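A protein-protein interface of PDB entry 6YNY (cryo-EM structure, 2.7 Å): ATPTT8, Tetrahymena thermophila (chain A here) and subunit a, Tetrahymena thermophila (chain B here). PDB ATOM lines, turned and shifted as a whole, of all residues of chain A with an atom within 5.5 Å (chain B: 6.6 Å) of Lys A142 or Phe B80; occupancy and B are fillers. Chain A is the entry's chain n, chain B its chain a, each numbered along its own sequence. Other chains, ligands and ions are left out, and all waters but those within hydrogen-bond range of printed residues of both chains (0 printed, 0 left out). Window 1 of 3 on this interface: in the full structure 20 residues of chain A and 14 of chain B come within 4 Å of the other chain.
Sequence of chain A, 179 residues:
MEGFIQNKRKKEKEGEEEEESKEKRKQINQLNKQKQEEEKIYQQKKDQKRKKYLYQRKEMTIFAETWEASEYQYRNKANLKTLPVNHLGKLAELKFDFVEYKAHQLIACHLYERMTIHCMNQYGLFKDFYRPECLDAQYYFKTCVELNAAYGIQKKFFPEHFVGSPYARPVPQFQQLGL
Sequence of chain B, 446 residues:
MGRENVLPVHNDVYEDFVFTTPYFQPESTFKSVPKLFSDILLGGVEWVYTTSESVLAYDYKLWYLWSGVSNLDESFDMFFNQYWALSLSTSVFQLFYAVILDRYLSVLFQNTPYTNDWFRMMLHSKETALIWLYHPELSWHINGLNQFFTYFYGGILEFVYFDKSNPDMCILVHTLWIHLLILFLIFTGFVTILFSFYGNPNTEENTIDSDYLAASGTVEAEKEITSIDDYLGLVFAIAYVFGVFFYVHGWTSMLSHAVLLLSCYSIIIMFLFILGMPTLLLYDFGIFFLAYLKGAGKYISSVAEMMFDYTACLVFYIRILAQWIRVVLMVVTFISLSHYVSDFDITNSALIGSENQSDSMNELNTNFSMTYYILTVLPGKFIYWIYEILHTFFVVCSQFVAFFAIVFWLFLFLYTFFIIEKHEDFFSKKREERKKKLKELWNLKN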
ATOM      1  N   ALA A 137       9.251  -7.292   0.523  1.00  0.00           N
ATOM      2  CA  ALA A 137      10.048  -6.693  -0.537  1.00  0.00           C
ATOM      3  C   ALA A 137      10.940  -5.591   0.012  1.00  0.00           C
ATOM      4  O   ALA A 137      12.103  -5.467  -0.384  1.00  0.00           O
ATOM      5  CB  ALA A 137       9.135  -6.151  -1.633  1.00  0.00           C
ATOM      6  N   GLN A 138      10.408  -4.779   0.925  1.00  0.00           N
ATOM      7  CA  GLN A 138      11.209  -3.743   1.557  1.00  0.00           C
ATOM      8  C   GLN A 138      12.310  -4.346   2.418  1.00  0.00           C
ATOM      9  O   GLN A 138      13.415  -3.799   2.497  1.00  0.00           O
ATOM     10  CB  GLN A 138      10.305  -2.841   2.391  1.00  0.00           C
ATOM     11  CG  GLN A 138      10.970  -1.601   2.920  1.00  0.00           C
ATOM     12  CD  GLN A 138      10.094  -0.854   3.896  1.00  0.00           C
ATOM     13  OE1 GLN A 138       9.077  -1.369   4.354  1.00  0.00           O
ATOM     14  NE2 GLN A 138      10.483   0.368   4.222  1.00  0.00           N
ATOM     15  N   TYR A 139      12.026  -5.470   3.078  1.00  0.00           N
ATOM     16  CA  TYR A 139      13.034  -6.107   3.917  1.00  0.00           C
ATOM     17  C   TYR A 139      14.098  -6.795   3.075  1.00  0.00           C
ATOM     18  O   TYR A 139      15.289  -6.724   3.392  1.00  0.00           O
ATOM     19  CB  TYR A 139      12.368  -7.101   4.864  1.00  0.00           C
ATOM     20  CG  TYR A 139      13.339  -7.919   5.674  1.00  0.00           C
ATOM     21  CD1 TYR A 139      14.027  -7.362   6.735  1.00  0.00           C
ATOM     22  CD2 TYR A 139      13.566  -9.251   5.378  1.00  0.00           C
ATOM     23  CE1 TYR A 139      14.915  -8.102   7.471  1.00  0.00           C
ATOM     24  CE2 TYR A 139      14.452  -9.999   6.110  1.00  0.00           C
ATOM     25  CZ  TYR A 139      15.124  -9.420   7.156  1.00  0.00           C
ATOM     26  OH  TYR A 139      16.011 -10.166   7.892  1.00  0.00           O
ATOM     27  N   TYR A 140      13.687  -7.469   2.001  1.00  0.00           N
ATOM     28  CA  TYR A 140      14.654  -8.104   1.115  1.00  0.00           C
ATOM     29  C   TYR A 140      15.573  -7.074   0.476  1.00  0.00           C
ATOM     30  O   TYR A 140      16.779  -7.304   0.341  1.00  0.00           O
ATOM     31  CB  TYR A 140      13.933  -8.908   0.040  1.00  0.00           C
ATOM     32  CG  TYR A 140      13.479 -10.282   0.463  1.00  0.00           C
ATOM     33  CD1 TYR A 140      13.321 -10.613   1.799  1.00  0.00           C
ATOM     34  CD2 TYR A 140      13.222 -11.258  -0.482  1.00  0.00           C
ATOM     35  CE1 TYR A 140      12.914 -11.870   2.171  1.00  0.00           C
ATOM     36  CE2 TYR A 140      12.815 -12.509  -0.118  1.00  0.00           C
ATOM     37  CZ  TYR A 140      12.661 -12.814   1.208  1.00  0.00           C
ATOM     38  OH  TYR A 140      12.255 -14.075   1.568  1.00  0.00           O
ATOM     39  N   PHE A 141      15.019  -5.932   0.074  1.00  0.00           N
ATOM     40  CA  PHE A 141      15.829  -4.897  -0.555  1.00  0.00           C
ATOM     41  C   PHE A 141      16.809  -4.290   0.437  1.00  0.00           C
ATOM     42  O   PHE A 141      17.991  -4.107   0.128  1.00  0.00           O
ATOM     43  CB  PHE A 141      14.923  -3.822  -1.147  1.00  0.00           C
ATOM     44  CG  PHE A 141      15.641  -2.569  -1.521  1.00  0.00           C
ATOM     45  CD1 PHE A 141      16.674  -2.594  -2.436  1.00  0.00           C
ATOM     46  CD2 PHE A 141      15.276  -1.362  -0.967  1.00  0.00           C
ATOM     47  CE1 PHE A 141      17.330  -1.446  -2.777  1.00  0.00           C
ATOM     48  CE2 PHE A 141      15.931  -0.211  -1.308  1.00  0.00           C
ATOM     49  CZ  PHE A 141      16.959  -0.251  -2.215  1.00  0.00           C
ATOM     50  N   LYS A 142      16.331  -3.970   1.638  1.00  0.00           N
ATOM     51  CA  LYS A 142      17.213  -3.431   2.663  1.00  0.00           C
ATOM     52  C   LYS A 142      18.276  -4.442   3.066  1.00  0.00           C
ATOM     53  O   LYS A 142      19.393  -4.057   3.425  1.00  0.00           O
ATOM     54  CB  LYS A 142      16.384  -3.001   3.869  1.00  0.00           C
ATOM     55  CG  LYS A 142      17.179  -2.480   5.039  1.00  0.00           C
ATOM     56  CD  LYS A 142      18.019  -1.283   4.664  1.00  0.00           C
ATOM     57  CE  LYS A 142      18.490  -0.554   5.901  1.00  0.00           C
ATOM     58  NZ  LYS A 142      19.503   0.472   5.586  1.00  0.00           N
ATOM     59  N   THR A 143      17.954  -5.731   3.009  1.00  0.00           N
ATOM     60  CA  THR A 143      18.890  -6.767   3.417  1.00  0.00           C
ATOM     61  C   THR A 143      19.833  -7.159   2.291  1.00  0.00           C
ATOM     62  O   THR A 143      20.991  -7.502   2.551  1.00  0.00           O
ATOM     63  CB  THR A 143      18.127  -8.004   3.898  1.00  0.00           C
ATOM     64  OG1 THR A 143      17.238  -7.642   4.960  1.00  0.00           O
ATOM     65  CG2 THR A 143      19.073  -9.061   4.390  1.00  0.00           C
ATOM     66  N   CYS A 144      19.358  -7.119   1.048  1.00  0.00           N
ATOM     67  CA  CYS A 144      20.192  -7.503  -0.083  1.00  0.00           C
ATOM     68  C   CYS A 144      21.347  -6.530  -0.272  1.00  0.00           C
ATOM     69  O   CYS A 144      22.484  -6.947  -0.516  1.00  0.00           O
ATOM     70  CB  CYS A 144      19.337  -7.586  -1.346  1.00  0.00           C
ATOM     71  SG  CYS A 144      20.141  -8.254  -2.803  1.00  0.00           S
ATOM     72  N   VAL A 145      21.078  -5.228  -0.157  1.00  0.00           N
ATOM     73  CA  VAL A 145      22.121  -4.233  -0.358  1.00  0.00           C
ATOM     74  C   VAL A 145      23.077  -4.177   0.821  1.00  0.00           C
ATOM     75  O   VAL A 145      24.210  -3.708   0.671  1.00  0.00           O
ATOM     76  CB  VAL A 145      21.504  -2.846  -0.624  1.00  0.00           C
ATOM     77  CG1 VAL A 145      20.603  -2.901  -1.821  1.00  0.00           C
ATOM     78  CG2 VAL A 145      20.738  -2.354   0.573  1.00  0.00           C
ATOM     79  N   GLU A 146      22.652  -4.642   1.993  1.00  0.00           N
ATOM     80  CA  GLU A 146      23.547  -4.691   3.141  1.00  0.00           C
ATOM     81  C   GLU A 146      24.519  -5.856   3.036  1.00  0.00           C
ATOM     82  O   GLU A 146      25.716  -5.695   3.291  1.00  0.00           O
ATOM     83  CB  GLU A 146      22.733  -4.791   4.427  1.00  0.00           C
ATOM     84  CG  GLU A 146      22.042  -3.508   4.807  1.00  0.00           C
ATOM     85  CD  GLU A 146      21.152  -3.661   6.023  1.00  0.00           C
ATOM     86  OE1 GLU A 146      20.807  -4.810   6.366  1.00  0.00           O
ATOM     87  OE2 GLU A 146      20.796  -2.635   6.636  1.00  0.00           O
ATOM     88  N   SER B  67      13.390  -5.064  12.308  1.00  0.00           N
ATOM     89  CA  SER B  67      12.859  -5.387  10.990  1.00  0.00           C
ATOM     90  C   SER B  67      13.224  -4.320   9.969  1.00  0.00           C
ATOM     91  O   SER B  67      13.488  -4.634   8.802  1.00  0.00           O
ATOM     92  CB  SER B  67      11.344  -5.551  11.069  1.00  0.00           C
ATOM     93  OG  SER B  67      10.732  -4.369  11.549  1.00  0.00           O
ATOM     94  N   GLY B  68      13.256  -3.060  10.387  1.00  0.00           N
ATOM     95  CA  GLY B  68      13.507  -1.969   9.479  1.00  0.00           C
ATOM     96  C   GLY B  68      12.333  -1.577   8.615  1.00  0.00           C
ATOM     97  O   GLY B  68      12.472  -0.665   7.789  1.00  0.00           O
ATOM     98  N   VAL B  69      11.182  -2.229   8.774  1.00  0.00           N
ATOM     99  CA  VAL B  69      10.005  -1.968   7.960  1.00  0.00           C
ATOM    100  C   VAL B  69       8.816  -1.517   8.797  1.00  0.00           C
ATOM    101  O   VAL B  69       7.701  -1.433   8.283  1.00  0.00           O
ATOM    102  CB  VAL B  69       9.633  -3.203   7.116  1.00  0.00           C
ATOM    103  CG1 VAL B  69      10.820  -3.657   6.301  1.00  0.00           C
ATOM    104  CG2 VAL B  69       9.135  -4.324   7.996  1.00  0.00           C
ATOM    105  N   ASP B  77      14.703   2.960   9.581  1.00  0.00           N
ATOM    106  CA  ASP B  77      15.817   3.768   9.089  1.00  0.00           C
ATOM    107  C   ASP B  77      15.243   4.895   8.244  1.00  0.00           C
ATOM    108  O   ASP B  77      14.994   4.744   7.048  1.00  0.00           O
ATOM    109  CB  ASP B  77      16.793   2.911   8.297  1.00  0.00           C
ATOM    110  CG  ASP B  77      18.121   3.604   8.068  1.00  0.00           C
ATOM    111  OD1 ASP B  77      18.136   4.845   7.953  1.00  0.00           O
ATOM    112  OD2 ASP B  77      19.154   2.906   8.008  1.00  0.00           O
ATOM    113  N   MET B  78      15.021   6.044   8.882  1.00  0.00           N
ATOM    114  CA  MET B  78      14.432   7.178   8.180  1.00  0.00           C
ATOM    115  C   MET B  78      15.398   7.757   7.154  1.00  0.00           C
ATOM    116  O   MET B  78      14.980   8.183   6.073  1.00  0.00           O
ATOM    117  CB  MET B  78      14.010   8.246   9.184  1.00  0.00           C
ATOM    118  CG  MET B  78      13.272   9.417   8.572  1.00  0.00           C
ATOM    119  SD  MET B  78      11.709   8.960   7.808  1.00  0.00           S
ATOM    120  CE  MET B  78      10.741   8.580   9.260  1.00  0.00           C
ATOM    121  N   PHE B  79      16.690   7.781   7.475  1.00  0.00           N
ATOM    122  CA  PHE B  79      17.673   8.325   6.545  1.00  0.00           C
ATOM    123  C   PHE B  79      17.715   7.519   5.256  1.00  0.00           C
ATOM    124  O   PHE B  79      17.633   8.078   4.156  1.00  0.00           O
ATOM    125  CB  PHE B  79      19.052   8.352   7.196  1.00  0.00           C
ATOM    126  CG  PHE B  79      20.156   8.685   6.244  1.00  0.00           C
ATOM    127  CD1 PHE B  79      20.371   9.987   5.847  1.00  0.00           C
ATOM    128  CD2 PHE B  79      20.977   7.697   5.742  1.00  0.00           C
ATOM    129  CE1 PHE B  79      21.381  10.294   4.973  1.00  0.00           C
ATOM    130  CE2 PHE B  79      21.985   8.002   4.867  1.00  0.00           C
ATOM    131  CZ  PHE B  79      22.187   9.301   4.482  1.00  0.00           C
ATOM    132  N   PHE B  80      17.847   6.200   5.372  1.00  0.00           N
ATOM    133  CA  PHE B  80      17.956   5.360   4.187  1.00  0.00           C
ATOM    134  C   PHE B  80      16.741   5.513   3.284  1.00  0.00           C
ATOM    135  O   PHE B  80      16.879   5.639   2.063  1.00  0.00           O
ATOM    136  CB  PHE B  80      18.135   3.905   4.606  1.00  0.00           C
ATOM    137  CG  PHE B  80      18.258   2.957   3.459  1.00  0.00           C
ATOM    138  CD1 PHE B  80      19.483   2.722   2.873  1.00  0.00           C
ATOM    139  CD2 PHE B  80      17.152   2.292   2.972  1.00  0.00           C
ATOM    140  CE1 PHE B  80      19.600   1.850   1.825  1.00  0.00           C
ATOM    141  CE2 PHE B  80      17.267   1.418   1.922  1.00  0.00           C
ATOM    142  CZ  PHE B  80      18.492   1.196   1.348  1.00  0.00           C
ATOM    143  N   ASN B  81      15.542   5.508   3.864  1.00  0.00           N
ATOM    144  CA  ASN B  81      14.336   5.579   3.050  1.00  0.00           C
ATOM    145  C   ASN B  81      14.144   6.966   2.451  1.00  0.00           C
ATOM    146  O   ASN B  81      13.678   7.096   1.313  1.00  0.00           O
ATOM    147  CB  ASN B  81      13.123   5.181   3.887  1.00  0.00           C
ATOM    148  CG  ASN B  81      13.099   3.706   4.214  1.00  0.00           C
ATOM    149  OD1 ASN B  81      12.651   2.889   3.414  1.00  0.00           O
ATOM    150  ND2 ASN B  81      13.576   3.356   5.397  1.00  0.00           N
ATOM    151  N   GLN B  82      14.497   8.013   3.194  1.00  0.00           N
ATOM    152  CA  GLN B  82      14.316   9.371   2.693  1.00  0.00           C
ATOM    153  C   GLN B  82      15.323   9.695   1.599  1.00  0.00           C
ATOM    154  O   GLN B  82      14.959  10.217   0.540  1.00  0.00           O
ATOM    155  CB  GLN B  82      14.437  10.369   3.837  1.00  0.00           C
ATOM    156  CG  GLN B  82      13.273  10.365   4.792  1.00  0.00           C
ATOM    157  CD  GLN B  82      11.995  10.851   4.158  1.00  0.00           C
ATOM    158  OE1 GLN B  82      11.998  11.379   3.048  1.00  0.00           O
ATOM    159  NE2 GLN B  82      10.890  10.678   4.863  1.00  0.00           N
ATOM    160  N   TYR B  83      16.600   9.401   1.840  1.00  0.00           N
ATOM    161  CA  TYR B  83      17.624   9.664   0.838  1.00  0.00           C
ATOM    162  C   TYR B  83      17.567   8.683  -0.323  1.00  0.00           C
ATOM    163  O   TYR B  83      18.050   9.006  -1.412  1.00  0.00           O
ATOM    164  CB  TYR B  83      19.007   9.638   1.485  1.00  0.00           C
ATOM    165  CG  TYR B  83      19.530  11.001   1.862  1.00  0.00           C
ATOM    166  CD1 TYR B  83      20.632  11.541   1.224  1.00  0.00           C
ATOM    167  CD2 TYR B  83      18.914  11.753   2.846  1.00  0.00           C
ATOM    168  CE1 TYR B  83      21.110  12.782   1.560  1.00  0.00           C
ATOM    169  CE2 TYR B  83      19.386  12.997   3.188  1.00  0.00           C
ATOM    170  CZ  TYR B  83      20.484  13.508   2.541  1.00  0.00           C
ATOM    171  OH  TYR B  83      20.959  14.750   2.879  1.00  0.00           O
ATOM    172  N   TRP B  84      16.990   7.500  -0.120  1.00  0.00           N
ATOM    173  CA  TRP B  84      16.749   6.600  -1.240  1.00  0.00           C
ATOM    174  C   TRP B  84      15.622   7.117  -2.120  1.00  0.00           C
ATOM    175  O   TRP B  84      15.777   7.233  -3.339  1.00  0.00           O
ATOM    176  CB  TRP B  84      16.427   5.199  -0.725  1.00  0.00           C
ATOM    177  CG  TRP B  84      15.887   4.292  -1.765  1.00  0.00           C
ATOM    178  CD1 TRP B  84      16.561   3.762  -2.819  1.00  0.00           C
ATOM    179  CD2 TRP B  84      14.549   3.799  -1.856  1.00  0.00           C
ATOM    180  NE1 TRP B  84      15.729   2.971  -3.563  1.00  0.00           N
ATOM    181  CE2 TRP B  84      14.485   2.977  -2.992  1.00  0.00           C
ATOM    182  CE3 TRP B  84      13.399   3.974  -1.086  1.00  0.00           C
ATOM    183  CZ2 TRP B  84      13.319   2.332  -3.377  1.00  0.00           C
ATOM    184  CZ3 TRP B  84      12.247   3.337  -1.469  1.00  0.00           C
ATOM    185  CH2 TRP B  84      12.212   2.524  -2.601  1.00  0.00           C
ATOM    186  N   ALA B  85      14.479   7.440  -1.515  1.00  0.00           N
ATOM    187  CA  ALA B  85      13.386   8.030  -2.274  1.00  0.00           C
ATOM    188  C   ALA B  85      13.801   9.344  -2.913  1.00  0.00           C
ATOM    189  O   ALA B  85      13.259   9.730  -3.955  1.00  0.00           O
ATOM    190  CB  ALA B  85      12.183   8.246  -1.361  1.00  0.00           C
ATOM    191  N   LEU B  86      14.749  10.045  -2.297  1.00  0.00           N
ATOM    192  CA  LEU B  86      15.248  11.289  -2.864  1.00  0.00           C
ATOM    193  C   LEU B  86      16.069  11.036  -4.122  1.00  0.00           C
ATOM    194  O   LEU B  86      16.004  11.814  -5.079  1.00  0.00           O
ATOM    195  CB  LEU B  86      16.072  12.018  -1.813  1.00  0.00           C
ATOM    196  CG  LEU B  86      16.622  13.388  -2.166  1.00  0.00           C
ATOM    197  CD1 LEU B  86      15.499  14.343  -2.466  1.00  0.00           C
ATOM    198  CD2 LEU B  86      17.450  13.880  -1.013  1.00  0.00           C
ATOM    199  N   LEU B 101      24.532   7.125   0.228  1.00  0.00           N
ATOM    200  CA  LEU B 101      23.894   5.901   0.696  1.00  0.00           C
ATOM    201  C   LEU B 101      24.880   4.743   0.743  1.00  0.00           C
ATOM    202  O   LEU B 101      24.858   3.940   1.682  1.00  0.00           O
ATOM    203  CB  LEU B 101      22.713   5.556  -0.205  1.00  0.00           C
ATOM    204  CG  LEU B 101      21.507   6.481  -0.116  1.00  0.00           C
ATOM    205  CD1 LEU B 101      20.576   6.229  -1.268  1.00  0.00           C
ATOM    206  CD2 LEU B 101      20.782   6.271   1.192  1.00  0.00           C
ATOM    207  N   TYR B 104      26.833   5.098   3.785  1.00  0.00           N
ATOM    208  CA  TYR B 104      26.050   4.770   4.967  1.00  0.00           C
ATOM    209  C   TYR B 104      25.997   3.267   5.193  1.00  0.00           C
ATOM    210  O   TYR B 104      25.982   2.813   6.342  1.00  0.00           O
ATOM    211  CB  TYR B 104      24.643   5.343   4.822  1.00  0.00           C
ATOM    212  CG  TYR B 104      23.701   4.983   5.943  1.00  0.00           C
ATOM    213  CD1 TYR B 104      23.757   5.644   7.156  1.00  0.00           C
ATOM    214  CD2 TYR B 104      22.746   3.993   5.782  1.00  0.00           C
ATOM    215  CE1 TYR B 104      22.899   5.324   8.177  1.00  0.00           C
ATOM    216  CE2 TYR B 104      21.886   3.667   6.800  1.00  0.00           C
ATOM    217  CZ  TYR B 104      21.965   4.335   7.995  1.00  0.00           C
ATOM    218  OH  TYR B 104      21.104   4.010   9.015  1.00  0.00           O
ATOM    219  N   LEU B 105      25.970   2.485   4.114  1.00  0.00           N
ATOM    220  CA  LEU B 105      25.981   1.035   4.242  1.00  0.00           C
ATOM    221  C   LEU B 105      27.337   0.515   4.694  1.00  0.00           C
ATOM    222  O   LEU B 105      27.409  -0.526   5.356  1.00  0.00           O
ATOM    223  CB  LEU B 105      25.589   0.396   2.914  1.00  0.00           C
ATOM    224  CG  LEU B 105      24.169   0.677   2.431  1.00  0.00           C
ATOM    225  CD1 LEU B 105      23.940   0.015   1.098  1.00  0.00           C
ATOM    226  CD2 LEU B 105      23.146   0.208   3.440  1.00  0.00           C
ATOM    227  N   LEU B 108      27.224   0.778   8.683  1.00  0.00           N
ATOM    228  CA  LEU B 108      26.527  -0.338   9.310  1.00  0.00           C
ATOM    229  C   LEU B 108      27.362  -1.606   9.275  1.00  0.00           C
ATOM    230  O   LEU B 108      27.236  -2.461  10.160  1.00  0.00           O
ATOM    231  CB  LEU B 108      25.199  -0.587   8.605  1.00  0.00           C
ATOM    232  CG  LEU B 108      24.197   0.556   8.542  1.00  0.00           C
ATOM    233  CD1 LEU B 108      23.001   0.097   7.745  1.00  0.00           C
ATOM    234  CD2 LEU B 108      23.789   1.006   9.926  1.00  0.00           C
ATOM    235  N   LEU B 133      19.733  12.819   8.784  1.00  0.00           N
ATOM    236  CA  LEU B 133      18.982  13.629   7.834  1.00  0.00           C
ATOM    237  C   LEU B 133      19.565  15.025   7.712  1.00  0.00           C
ATOM    238  O   LEU B 133      19.398  15.681   6.678  1.00  0.00           O
ATOM    239  CB  LEU B 133      17.521  13.711   8.263  1.00  0.00           C
ATOM    240  CG  LEU B 133      16.799  12.381   8.454  1.00  0.00           C
ATOM    241  CD1 LEU B 133      15.473  12.607   9.125  1.00  0.00           C
ATOM    242  CD2 LEU B 133      16.610  11.680   7.129  1.00  0.00           C
ATOM    243  N   LYS B 164      20.032  -9.505  14.069  1.00  0.00           N
ATOM    244  CA  LYS B 164      19.083  -8.417  14.251  1.00  0.00           C
ATOM    245  C   LYS B 164      18.034  -8.743  15.299  1.00  0.00           C
ATOM    246  O   LYS B 164      17.449  -7.824  15.881  1.00  0.00           O
ATOM    247  CB  LYS B 164      18.395  -8.086  12.927  1.00  0.00           C
ATOM    248  CG  LYS B 164      19.312  -7.550  11.851  1.00  0.00           C
ATOM    249  CD  LYS B 164      19.919  -6.232  12.251  1.00  0.00           C
ATOM    250  CE  LYS B 164      20.599  -5.558  11.079  1.00  0.00           C
ATOM    251  NZ  LYS B 164      19.622  -5.148  10.039  1.00  0.00           N
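The backbone NH of Phe B79 is in hydrogen-bond range of the side-chain carboxylate of Asp B77 (3.3 Å). N of Phe B80 is in hydrogen-bond range of OD1 of Asp B77. O of Asp B77 sits at hydrogen-bond distance from ND2 of Asn B81, 2.6 Å away. OD2 of Asp B77 lies within hydrogen-bond range of OH of Tyr B104 (2.5 Å). The backbone carbonyl oxygen (O) of Tyr A139 lies within hydrogen-bond range of the side-chain hydroxyl (OG1) of Thr A143 (2.7 Å). The side-chain carboxylate of Glu A146 lies within salt-bridge range of the side-chain amino group of Lys A142.
The side-chain carboxylate (OD2) of Asp B77 is in salt-bridge range of the side-chain amino group (NZ) of Lys A142, at 3.5 Å. NE2 of Gln A138 lies within hydrogen-bond range of OD1 of Asn B81, 3.4 Å away. The side-chain amino group of Lys B164 lies within salt-bridge range of the side-chain carboxylate of Glu A146, at 3.9 Å.
Of the 19 printed residues of chain B, 9 touch a printed residue of chain A. Hydrophobic or aromatic side chains of chain B within 4 Å of the printed part of chain A: Val B69, Phe B80, Trp B84, Leu B105 and Leu B108. Hydrophobic or aromatic side chains of chain A that line the printed part of chain B: Tyr A139 and Phe A141.
CB of Val B69 touches OE1 of Gln A138 (3.4 Å). O of Ser B67 touches CD1 of Tyr A139, 3.5 Å away. Tyr A139 touches Val B69. Phe A141 touches Phe B80. Trp B84 touches Phe A141. Phe B80 touches Lys A142. Val A145 touches Leu B105. OE2 of Glu A146 touches CD1 of Leu B108 (3.7 Å).
Of the printed residues of chain B, Lys A142 touches Asp B77 (3.5 Å) and Phe B80 (3.5 Å). Of the printed residues of chain A, Asp B77 touches Lys A142 (3.5 Å). Phe B80 touches two residues of chain A. Of the printed residues of chain A, Leu B108 touches Glu A146. Leu B133 touches none of the printed residues of chain A. Of the printed residues of chain A, Lys B164 touches Glu A146 (3.9 Å). The nearest residue of chain B that does not touch Lys A142 is Leu B108 (4.1 Å). The nearest residue of chain A that does not touch Phe B80 is Val A145 (4.3 Å). The nearest printed residue of chain A that does not touch Lys B164 is Tyr A139 (5.8 Å).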
